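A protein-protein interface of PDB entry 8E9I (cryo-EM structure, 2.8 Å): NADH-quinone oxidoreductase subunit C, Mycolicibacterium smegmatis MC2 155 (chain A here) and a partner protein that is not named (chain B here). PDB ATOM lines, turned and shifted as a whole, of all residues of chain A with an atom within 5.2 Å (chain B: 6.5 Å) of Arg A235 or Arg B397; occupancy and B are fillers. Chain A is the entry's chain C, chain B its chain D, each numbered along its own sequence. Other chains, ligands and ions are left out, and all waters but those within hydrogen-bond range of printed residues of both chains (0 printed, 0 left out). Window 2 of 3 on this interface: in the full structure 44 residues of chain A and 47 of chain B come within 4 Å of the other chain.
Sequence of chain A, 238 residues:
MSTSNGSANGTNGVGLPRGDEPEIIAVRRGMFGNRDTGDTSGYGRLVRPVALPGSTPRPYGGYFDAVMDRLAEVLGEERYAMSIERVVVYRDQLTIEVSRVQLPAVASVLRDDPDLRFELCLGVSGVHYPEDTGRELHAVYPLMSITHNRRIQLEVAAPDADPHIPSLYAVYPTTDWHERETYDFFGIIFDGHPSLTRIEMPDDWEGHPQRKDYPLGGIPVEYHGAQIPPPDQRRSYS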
ATOM      1  N   ASN A  34      13.563   8.505   8.509  1.00  0.00           N
ATOM      2  CA  ASN A  34      14.570   8.834   7.513  1.00  0.00           C
ATOM      3  C   ASN A  34      15.484   9.925   8.045  1.00  0.00           C
ATOM      4  O   ASN A  34      15.019  10.952   8.543  1.00  0.00           O
ATOM      5  CB  ASN A  34      13.916   9.297   6.214  1.00  0.00           C
ATOM      6  CG  ASN A  34      13.496   8.145   5.337  1.00  0.00           C
ATOM      7  OD1 ASN A  34      14.328   7.360   4.889  1.00  0.00           O
ATOM      8  ND2 ASN A  34      12.203   8.051   5.062  1.00  0.00           N
ATOM      9  N   ARG A  35      16.791   9.691   7.949  1.00  0.00           N
ATOM     10  CA  ARG A  35      17.750  10.729   8.297  1.00  0.00           C
ATOM     11  C   ARG A  35      17.988  11.688   7.141  1.00  0.00           C
ATOM     12  O   ARG A  35      18.592  12.745   7.340  1.00  0.00           O
ATOM     13  CB  ARG A  35      19.070  10.096   8.735  1.00  0.00           C
ATOM     14  N   ASP A  36      17.501  11.356   5.945  1.00  0.00           N
ATOM     15  CA  ASP A  36      17.669  12.204   4.772  1.00  0.00           C
ATOM     16  C   ASP A  36      16.432  12.100   3.889  1.00  0.00           C
ATOM     17  O   ASP A  36      15.378  11.660   4.355  1.00  0.00           O
ATOM     18  CB  ASP A  36      18.942  11.830   4.007  1.00  0.00           C
ATOM     19  CG  ASP A  36      18.997  10.365   3.639  1.00  0.00           C
ATOM     20  OD1 ASP A  36      17.945   9.698   3.658  1.00  0.00           O
ATOM     21  OD2 ASP A  36      20.104   9.879   3.323  1.00  0.00           O
ATOM     22  N   GLY A  38      14.736  10.380   1.976  1.00  0.00           N
ATOM     23  CA  GLY A  38      13.792   9.293   2.123  1.00  0.00           C
ATOM     24  C   GLY A  38      13.597   8.502   0.842  1.00  0.00           C
ATOM     25  O   GLY A  38      13.728   9.005  -0.272  1.00  0.00           O
ATOM     26  N   ASP A  39      13.260   7.224   1.023  1.00  0.00           N
ATOM     27  CA  ASP A  39      13.221   6.285  -0.088  1.00  0.00           C
ATOM     28  C   ASP A  39      11.877   6.253  -0.799  1.00  0.00           C
ATOM     29  O   ASP A  39      11.761   5.596  -1.837  1.00  0.00           O
ATOM     30  CB  ASP A  39      13.571   4.885   0.411  1.00  0.00           C
ATOM     31  N   PRO A 231      28.936   0.260   9.788  1.00  0.00           N
ATOM     32  CA  PRO A 231      27.527   0.630   9.979  1.00  0.00           C
ATOM     33  C   PRO A 231      27.258   2.123   9.914  1.00  0.00           C
ATOM     34  O   PRO A 231      26.126   2.507   9.599  1.00  0.00           O
ATOM     35  CB  PRO A 231      27.212   0.074  11.370  1.00  0.00           C
ATOM     36  CG  PRO A 231      28.517   0.048  12.055  1.00  0.00           C
ATOM     37  CD  PRO A 231      29.506  -0.342  11.000  1.00  0.00           C
ATOM     38  N   GLN A 233      28.328   4.265   7.796  1.00  0.00           N
ATOM     39  CA  GLN A 233      28.226   4.757   6.429  1.00  0.00           C
ATOM     40  C   GLN A 233      26.929   4.314   5.771  1.00  0.00           C
ATOM     41  O   GLN A 233      26.334   5.067   4.996  1.00  0.00           O
ATOM     42  CB  GLN A 233      29.416   4.269   5.614  1.00  0.00           C
ATOM     43  CG  GLN A 233      30.749   4.675   6.185  1.00  0.00           C
ATOM     44  CD  GLN A 233      31.897   4.281   5.293  1.00  0.00           C
ATOM     45  OE1 GLN A 233      31.699   3.882   4.151  1.00  0.00           O
ATOM     46  NE2 GLN A 233      33.111   4.392   5.811  1.00  0.00           N
ATOM     47  N   ARG A 234      26.479   3.102   6.065  1.00  0.00           N
ATOM     48  CA  ARG A 234      25.309   2.562   5.404  1.00  0.00           C
ATOM     49  C   ARG A 234      24.040   3.180   5.971  1.00  0.00           C
ATOM     50  O   ARG A 234      24.043   3.838   7.012  1.00  0.00           O
ATOM     51  CB  ARG A 234      25.279   1.047   5.543  1.00  0.00           C
ATOM     52  CG  ARG A 234      26.574   0.387   5.102  1.00  0.00           C
ATOM     53  CD  ARG A 234      26.409  -1.097   4.944  1.00  0.00           C
ATOM     54  NE  ARG A 234      25.491  -1.619   5.945  1.00  0.00           N
ATOM     55  CZ  ARG A 234      25.853  -2.085   7.130  1.00  0.00           C
ATOM     56  NH1 ARG A 234      27.119  -2.113   7.506  1.00  0.00           N
ATOM     57  NH2 ARG A 234      24.917  -2.522   7.965  1.00  0.00           N
ATOM     58  N   ARG A 235      22.941   2.950   5.260  1.00  0.00           N
ATOM     59  CA  ARG A 235      21.685   3.618   5.559  1.00  0.00           C
ATOM     60  C   ARG A 235      21.139   3.192   6.916  1.00  0.00           C
ATOM     61  O   ARG A 235      21.440   2.110   7.425  1.00  0.00           O
ATOM     62  CB  ARG A 235      20.665   3.313   4.466  1.00  0.00           C
ATOM     63  CG  ARG A 235      19.427   4.162   4.551  1.00  0.00           C
ATOM     64  CD  ARG A 235      18.679   4.198   3.238  1.00  0.00           C
ATOM     65  NE  ARG A 235      17.582   5.149   3.307  1.00  0.00           N
ATOM     66  CZ  ARG A 235      17.741   6.463   3.383  1.00  0.00           C
ATOM     67  NH1 ARG A 235      18.940   7.015   3.360  1.00  0.00           N
ATOM     68  NH2 ARG A 235      16.668   7.240   3.487  1.00  0.00           N
ATOM     69  N   SER A 236      20.328   4.069   7.503  1.00  0.00           N
ATOM     70  CA  SER A 236      19.748   3.825   8.813  1.00  0.00           C
ATOM     71  C   SER A 236      18.425   4.563   8.913  1.00  0.00           C
ATOM     72  O   SER A 236      18.152   5.494   8.154  1.00  0.00           O
ATOM     73  CB  SER A 236      20.677   4.287   9.935  1.00  0.00           C
ATOM     74  OG  SER A 236      20.879   5.684   9.863  1.00  0.00           O
ATOM     75  N   TYR A 237      17.607   4.138   9.869  1.00  0.00           N
ATOM     76  CA  TYR A 237      16.340   4.800  10.132  1.00  0.00           C
ATOM     77  C   TYR A 237      16.121   4.945  11.631  1.00  0.00           C
ATOM     78  O   TYR A 237      14.994   4.886  12.112  1.00  0.00           O
ATOM     79  CB  TYR A 237      15.194   4.022   9.497  1.00  0.00           C
ATOM     80  CG  TYR A 237      15.351   3.843   8.006  1.00  0.00           C
ATOM     81  CD1 TYR A 237      16.071   2.778   7.491  1.00  0.00           C
ATOM     82  CD2 TYR A 237      14.787   4.741   7.116  1.00  0.00           C
ATOM     83  CE1 TYR A 237      16.225   2.611   6.135  1.00  0.00           C
ATOM     84  CE2 TYR A 237      14.934   4.580   5.757  1.00  0.00           C
ATOM     85  CZ  TYR A 237      15.652   3.513   5.273  1.00  0.00           C
ATOM     86  OH  TYR A 237      15.802   3.353   3.919  1.00  0.00           O
ATOM     87  N   LEU B  85      27.809   0.633  19.843  1.00  0.00           N
ATOM     88  CA  LEU B  85      26.401   0.378  20.107  1.00  0.00           C
ATOM     89  C   LEU B  85      25.511   1.313  19.310  1.00  0.00           C
ATOM     90  O   LEU B  85      24.488   0.895  18.765  1.00  0.00           O
ATOM     91  CB  LEU B  85      26.102   0.560  21.593  1.00  0.00           C
ATOM     92  CG  LEU B  85      26.493  -0.578  22.522  1.00  0.00           C
ATOM     93  CD1 LEU B  85      26.557  -0.092  23.952  1.00  0.00           C
ATOM     94  CD2 LEU B  85      25.491  -1.696  22.397  1.00  0.00           C
ATOM     95  N   GLU B  86      25.901   2.582  19.229  1.00  0.00           N
ATOM     96  CA  GLU B  86      25.007   3.599  18.699  1.00  0.00           C
ATOM     97  C   GLU B  86      24.642   3.359  17.244  1.00  0.00           C
ATOM     98  O   GLU B  86      23.694   3.976  16.752  1.00  0.00           O
ATOM     99  CB  GLU B  86      25.645   4.976  18.860  1.00  0.00           C
ATOM    100  CG  GLU B  86      25.997   5.302  20.296  1.00  0.00           C
ATOM    101  CD  GLU B  86      26.671   6.644  20.442  1.00  0.00           C
ATOM    102  OE1 GLU B  86      26.748   7.380  19.439  1.00  0.00           O
ATOM    103  OE2 GLU B  86      27.126   6.962  21.559  1.00  0.00           O
ATOM    104  N   TYR B  87      25.365   2.493  16.545  1.00  0.00           N
ATOM    105  CA  TYR B  87      25.087   2.200  15.148  1.00  0.00           C
ATOM    106  C   TYR B  87      24.388   0.865  14.963  1.00  0.00           C
ATOM    107  O   TYR B  87      24.449   0.287  13.875  1.00  0.00           O
ATOM    108  CB  TYR B  87      26.384   2.238  14.346  1.00  0.00           C
ATOM    109  CG  TYR B  87      27.057   3.583  14.423  1.00  0.00           C
ATOM    110  CD1 TYR B  87      26.720   4.601  13.549  1.00  0.00           C
ATOM    111  CD2 TYR B  87      28.014   3.841  15.385  1.00  0.00           C
ATOM    112  CE1 TYR B  87      27.321   5.831  13.628  1.00  0.00           C
ATOM    113  CE2 TYR B  87      28.620   5.067  15.468  1.00  0.00           C
ATOM    114  CZ  TYR B  87      28.271   6.057  14.588  1.00  0.00           C
ATOM    115  OH  TYR B  87      28.879   7.282  14.671  1.00  0.00           O
ATOM    116  N   ARG B  88      23.728   0.364  16.001  1.00  0.00           N
ATOM    117  CA  ARG B  88      23.009  -0.897  15.959  1.00  0.00           C
ATOM    118  C   ARG B  88      21.662  -0.705  16.634  1.00  0.00           C
ATOM    119  O   ARG B  88      21.461   0.258  17.371  1.00  0.00           O
ATOM    120  CB  ARG B  88      23.794  -2.003  16.659  1.00  0.00           C
ATOM    121  CG  ARG B  88      25.186  -2.214  16.107  1.00  0.00           C
ATOM    122  CD  ARG B  88      25.132  -2.762  14.705  1.00  0.00           C
ATOM    123  NE  ARG B  88      26.457  -2.980  14.145  1.00  0.00           N
ATOM    124  CZ  ARG B  88      26.684  -3.308  12.882  1.00  0.00           C
ATOM    125  NH1 ARG B  88      25.694  -3.452  12.018  1.00  0.00           N
ATOM    126  NH2 ARG B  88      27.935  -3.499  12.477  1.00  0.00           N
ATOM    127  N   ASN B  89      20.730  -1.612  16.369  1.00  0.00           N
ATOM    128  CA  ASN B  89      19.413  -1.463  16.961  1.00  0.00           C
ATOM    129  C   ASN B  89      19.415  -1.966  18.400  1.00  0.00           C
ATOM    130  O   ASN B  89      20.393  -2.533  18.887  1.00  0.00           O
ATOM    131  CB  ASN B  89      18.363  -2.214  16.147  1.00  0.00           C
ATOM    132  CG  ASN B  89      18.664  -3.687  16.028  1.00  0.00           C
ATOM    133  OD1 ASN B  89      19.638  -4.084  15.398  1.00  0.00           O
ATOM    134  ND2 ASN B  89      17.830  -4.509  16.643  1.00  0.00           N
ATOM    135  N   TRP B  90      18.303  -1.723  19.091  1.00  0.00           N
ATOM    136  CA  TRP B  90      18.057  -2.373  20.370  1.00  0.00           C
ATOM    137  C   TRP B  90      17.920  -3.860  20.098  1.00  0.00           C
ATOM    138  O   TRP B  90      17.595  -4.253  18.974  1.00  0.00           O
ATOM    139  CB  TRP B  90      16.787  -1.852  21.042  1.00  0.00           C
ATOM    140  CG  TRP B  90      16.624  -0.374  21.031  1.00  0.00           C
ATOM    141  CD1 TRP B  90      15.969   0.359  20.101  1.00  0.00           C
ATOM    142  CD2 TRP B  90      17.101   0.551  22.009  1.00  0.00           C
ATOM    143  NE1 TRP B  90      16.015   1.689  20.423  1.00  0.00           N
ATOM    144  CE2 TRP B  90      16.707   1.833  21.594  1.00  0.00           C
ATOM    145  CE3 TRP B  90      17.829   0.423  23.192  1.00  0.00           C
ATOM    146  CZ2 TRP B  90      17.009   2.974  22.320  1.00  0.00           C
ATOM    147  CZ3 TRP B  90      18.132   1.556  23.906  1.00  0.00           C
ATOM    148  CH2 TRP B  90      17.723   2.816  23.470  1.00  0.00           C
ATOM    149  N   GLU B 366      14.680  -3.500  11.457  1.00  0.00           N
ATOM    150  CA  GLU B 366      14.746  -2.185  12.080  1.00  0.00           C
ATOM    151  C   GLU B 366      14.783  -2.306  13.593  1.00  0.00           C
ATOM    152  O   GLU B 366      15.545  -1.600  14.258  1.00  0.00           O
ATOM    153  CB  GLU B 366      13.555  -1.335  11.643  1.00  0.00           C
ATOM    154  N   ILE B 368      12.516  -2.609  17.413  1.00  0.00           N
ATOM    155  CA  ILE B 368      11.670  -1.671  18.125  1.00  0.00           C
ATOM    156  C   ILE B 368      12.334  -0.301  18.155  1.00  0.00           C
ATOM    157  O   ILE B 368      13.563  -0.173  18.134  1.00  0.00           O
ATOM    158  CB  ILE B 368      11.394  -2.170  19.549  1.00  0.00           C
ATOM    159  CG1 ILE B 368      12.708  -2.339  20.311  1.00  0.00           C
ATOM    160  CG2 ILE B 368      10.674  -3.489  19.499  1.00  0.00           C
ATOM    161  CD1 ILE B 368      12.525  -2.628  21.769  1.00  0.00           C
ATOM    162  N   ARG B 369      11.509   0.735  18.201  1.00  0.00           N
ATOM    163  CA  ARG B 369      11.979   2.082  18.466  1.00  0.00           C
ATOM    164  C   ARG B 369      11.459   2.503  19.830  1.00  0.00           C
ATOM    165  O   ARG B 369      10.261   2.404  20.108  1.00  0.00           O
ATOM    166  CB  ARG B 369      11.533   3.067  17.383  1.00  0.00           C
ATOM    167  CG  ARG B 369      10.053   3.123  17.132  1.00  0.00           C
ATOM    168  CD  ARG B 369       9.751   4.040  15.957  1.00  0.00           C
ATOM    169  NE  ARG B 369      10.328   3.527  14.718  1.00  0.00           N
ATOM    170  CZ  ARG B 369      10.694   4.272  13.683  1.00  0.00           C
ATOM    171  NH1 ARG B 369      10.571   5.589  13.698  1.00  0.00           N
ATOM    172  NH2 ARG B 369      11.188   3.678  12.601  1.00  0.00           N
ATOM    173  N   VAL B 391      20.042   6.339  27.018  1.00  0.00           N
ATOM    174  CA  VAL B 391      19.389   7.490  26.416  1.00  0.00           C
ATOM    175  C   VAL B 391      18.863   7.070  25.057  1.00  0.00           C
ATOM    176  O   VAL B 391      19.603   6.494  24.251  1.00  0.00           O
ATOM    177  CB  VAL B 391      20.341   8.687  26.269  1.00  0.00           C
ATOM    178  CG1 VAL B 391      19.588   9.899  25.772  1.00  0.00           C
ATOM    179  CG2 VAL B 391      21.035   8.979  27.579  1.00  0.00           C
ATOM    180  N   SER B 392      17.595   7.368  24.804  1.00  0.00           N
ATOM    181  CA  SER B 392      16.925   7.064  23.555  1.00  0.00           C
ATOM    182  C   SER B 392      16.468   8.356  22.900  1.00  0.00           C
ATOM    183  O   SER B 392      15.968   9.261  23.576  1.00  0.00           O
ATOM    184  CB  SER B 392      15.724   6.153  23.796  1.00  0.00           C
ATOM    185  OG  SER B 392      14.990   5.969  22.603  1.00  0.00           O
ATOM    186  N   ASP B 393      16.646   8.440  21.584  1.00  0.00           N
ATOM    187  CA  ASP B 393      16.197   9.581  20.800  1.00  0.00           C
ATOM    188  C   ASP B 393      14.954   9.255  19.985  1.00  0.00           C
ATOM    189  O   ASP B 393      14.732   9.846  18.924  1.00  0.00           O
ATOM    190  CB  ASP B 393      17.318  10.063  19.882  1.00  0.00           C
ATOM    191  N   GLY B 394      14.143   8.313  20.452  1.00  0.00           N
ATOM    192  CA  GLY B 394      12.974   7.898  19.714  1.00  0.00           C
ATOM    193  C   GLY B 394      13.257   6.953  18.571  1.00  0.00           C
ATOM    194  O   GLY B 394      12.315   6.534  17.890  1.00  0.00           O
ATOM    195  N   GLY B 395      14.519   6.595  18.342  1.00  0.00           N
ATOM    196  CA  GLY B 395      14.886   5.791  17.201  1.00  0.00           C
ATOM    197  C   GLY B 395      15.053   4.327  17.545  1.00  0.00           C
ATOM    198  O   GLY B 395      14.941   3.903  18.691  1.00  0.00           O
ATOM    199  N   THR B 396      15.326   3.546  16.509  1.00  0.00           N
ATOM    200  CA  THR B 396      15.538   2.118  16.669  1.00  0.00           C
ATOM    201  C   THR B 396      16.940   1.780  17.138  1.00  0.00           C
ATOM    202  O   THR B 396      17.194   0.628  17.498  1.00  0.00           O
ATOM    203  CB  THR B 396      15.273   1.402  15.350  1.00  0.00           C
ATOM    204  OG1 THR B 396      16.178   1.893  14.355  1.00  0.00           O
ATOM    205  CG2 THR B 396      13.848   1.643  14.900  1.00  0.00           C
ATOM    206  N   ARG B 397      17.851   2.743  17.126  1.00  0.00           N
ATOM    207  CA  ARG B 397      19.175   2.541  17.682  1.00  0.00           C
ATOM    208  C   ARG B 397      19.315   3.319  18.978  1.00  0.00           C
ATOM    209  O   ARG B 397      18.759   4.412  19.104  1.00  0.00           O
ATOM    210  CB  ARG B 397      20.256   3.008  16.708  1.00  0.00           C
ATOM    211  CG  ARG B 397      20.232   2.320  15.369  1.00  0.00           C
ATOM    212  CD  ARG B 397      21.302   2.882  14.461  1.00  0.00           C
ATOM    213  NE  ARG B 397      21.447   2.097  13.244  1.00  0.00           N
ATOM    214  CZ  ARG B 397      22.350   2.333  12.305  1.00  0.00           C
ATOM    215  NH1 ARG B 397      23.213   3.329  12.409  1.00  0.00           N
ATOM    216  NH2 ARG B 397      22.385   1.551  11.231  1.00  0.00           N
ATOM    217  N   PRO B 398      20.050   2.807  19.958  1.00  0.00           N
ATOM    218  CA  PRO B 398      20.247   3.575  21.185  1.00  0.00           C
ATOM    219  C   PRO B 398      20.985   4.867  20.894  1.00  0.00           C
ATOM    220  O   PRO B 398      21.877   4.919  20.048  1.00  0.00           O
ATOM    221  CB  PRO B 398      21.072   2.633  22.061  1.00  0.00           C
ATOM    222  CG  PRO B 398      21.811   1.811  21.118  1.00  0.00           C
ATOM    223  CD  PRO B 398      20.953   1.651  19.897  1.00  0.00           C
ATOM    224  N   TYR B 399      20.590   5.926  21.596  1.00  0.00           N
ATOM    225  CA  TYR B 399      21.318   7.179  21.481  1.00  0.00           C
ATOM    226  C   TYR B 399      22.551   7.175  22.370  1.00  0.00           C
ATOM    227  O   TYR B 399      23.598   7.705  21.988  1.00  0.00           O
ATOM    228  CB  TYR B 399      20.408   8.348  21.836  1.00  0.00           C
ATOM    229  CG  TYR B 399      20.996   9.679  21.463  1.00  0.00           C
ATOM    230  CD1 TYR B 399      20.889  10.171  20.174  1.00  0.00           C
ATOM    231  CD2 TYR B 399      21.672  10.440  22.398  1.00  0.00           C
ATOM    232  CE1 TYR B 399      21.429  11.383  19.833  1.00  0.00           C
ATOM    233  CE2 TYR B 399      22.218  11.651  22.064  1.00  0.00           C
ATOM    234  CZ  TYR B 399      22.098  12.119  20.781  1.00  0.00           C
ATOM    235  OH  TYR B 399      22.642  13.334  20.448  1.00  0.00           O
ATOM    236  N   ARG B 400      22.447   6.578  23.551  1.00  0.00           N
ATOM    237  CA  ARG B 400      23.582   6.478  24.454  1.00  0.00           C
ATOM    238  C   ARG B 400      23.400   5.264  25.343  1.00  0.00           C
ATOM    239  O   ARG B 400      22.313   5.035  25.870  1.00  0.00           O
ATOM    240  CB  ARG B 400      23.716   7.735  25.311  1.00  0.00           C
ATOM    241  CG  ARG B 400      24.912   7.774  26.234  1.00  0.00           C
ATOM    242  CD  ARG B 400      26.182   8.106  25.499  1.00  0.00           C
ATOM    243  NE  ARG B 400      27.336   8.040  26.388  1.00  0.00           N
ATOM    244  CZ  ARG B 400      28.361   7.211  26.253  1.00  0.00           C
ATOM    245  NH1 ARG B 400      28.416   6.325  25.274  1.00  0.00           N
ATOM    246  NH2 ARG B 400      29.360   7.275  27.125  1.00  0.00           N
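The guanidinium group (NH2) of Arg A235 sits at hydrogen-bond distance from the side-chain amide oxygen (OD1) of Asn A34 (2.7 Å). The guanidinium group of Arg A235 is in salt-bridge range of the side-chain carboxylate of Asp A36, at 2.8 Å. The guanidinium group (NE) of Arg A235 sits at hydrogen-bond distance from the side-chain hydroxyl (OH) of Tyr A237 (2.6 Å). N of Trp B90 sits close to O of Thr B396, at 3.0 Å.
Among the printed residues, merely in contact across the chains: Pro A231 with Tyr B87 (3.7 Å), Pro A231 with Arg B88 (3.6 Å), Arg A235 with Arg B397 (3.96 Å), Ser A236 with Arg B397 (3.5 Å) and Tyr A237 with Thr B396 (3.9 Å).
Of chain B, only Arg B397 comes within 4 Å of Arg A235. Of chain A, only Arg A235 (3.96 Å) and Ser A236 (3.5 Å) come within 4 Å of Arg B397. Printed residues of chain A within 4 Å of Thr B396: Tyr A237 (3.9 Å). Printed residues of chain B within 4 Å of Pro A231: Tyr B87 and Arg B88. Of the printed residues of chain A, Arg B88 touches Pro A231 (3.6 Å). Of the printed residues of chain A, Tyr B87 touches Pro A231. Of the printed residues of chain B, Ser A236 touches Arg B397 (3.5 Å). Pro B398 touches none of the printed residues of chain A. Asp A36 touches none of the printed residues of chain B. The nearest residue of chain A that does not touch Arg B397 is Pro A231 (4.1 Å). The nearest printed residue of chain B that does not touch Pro A231 is Arg B397 (4.1 Å).
Of the 19 printed residues of chain B, 4 touch a printed residue of chain A. Among the printed residues, 5 pairs touch across the chains. Among the printed residues, no Asp or Glu carboxylate lies within 4 Å of a Lys or Arg side-chain nitrogen of the other chain.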
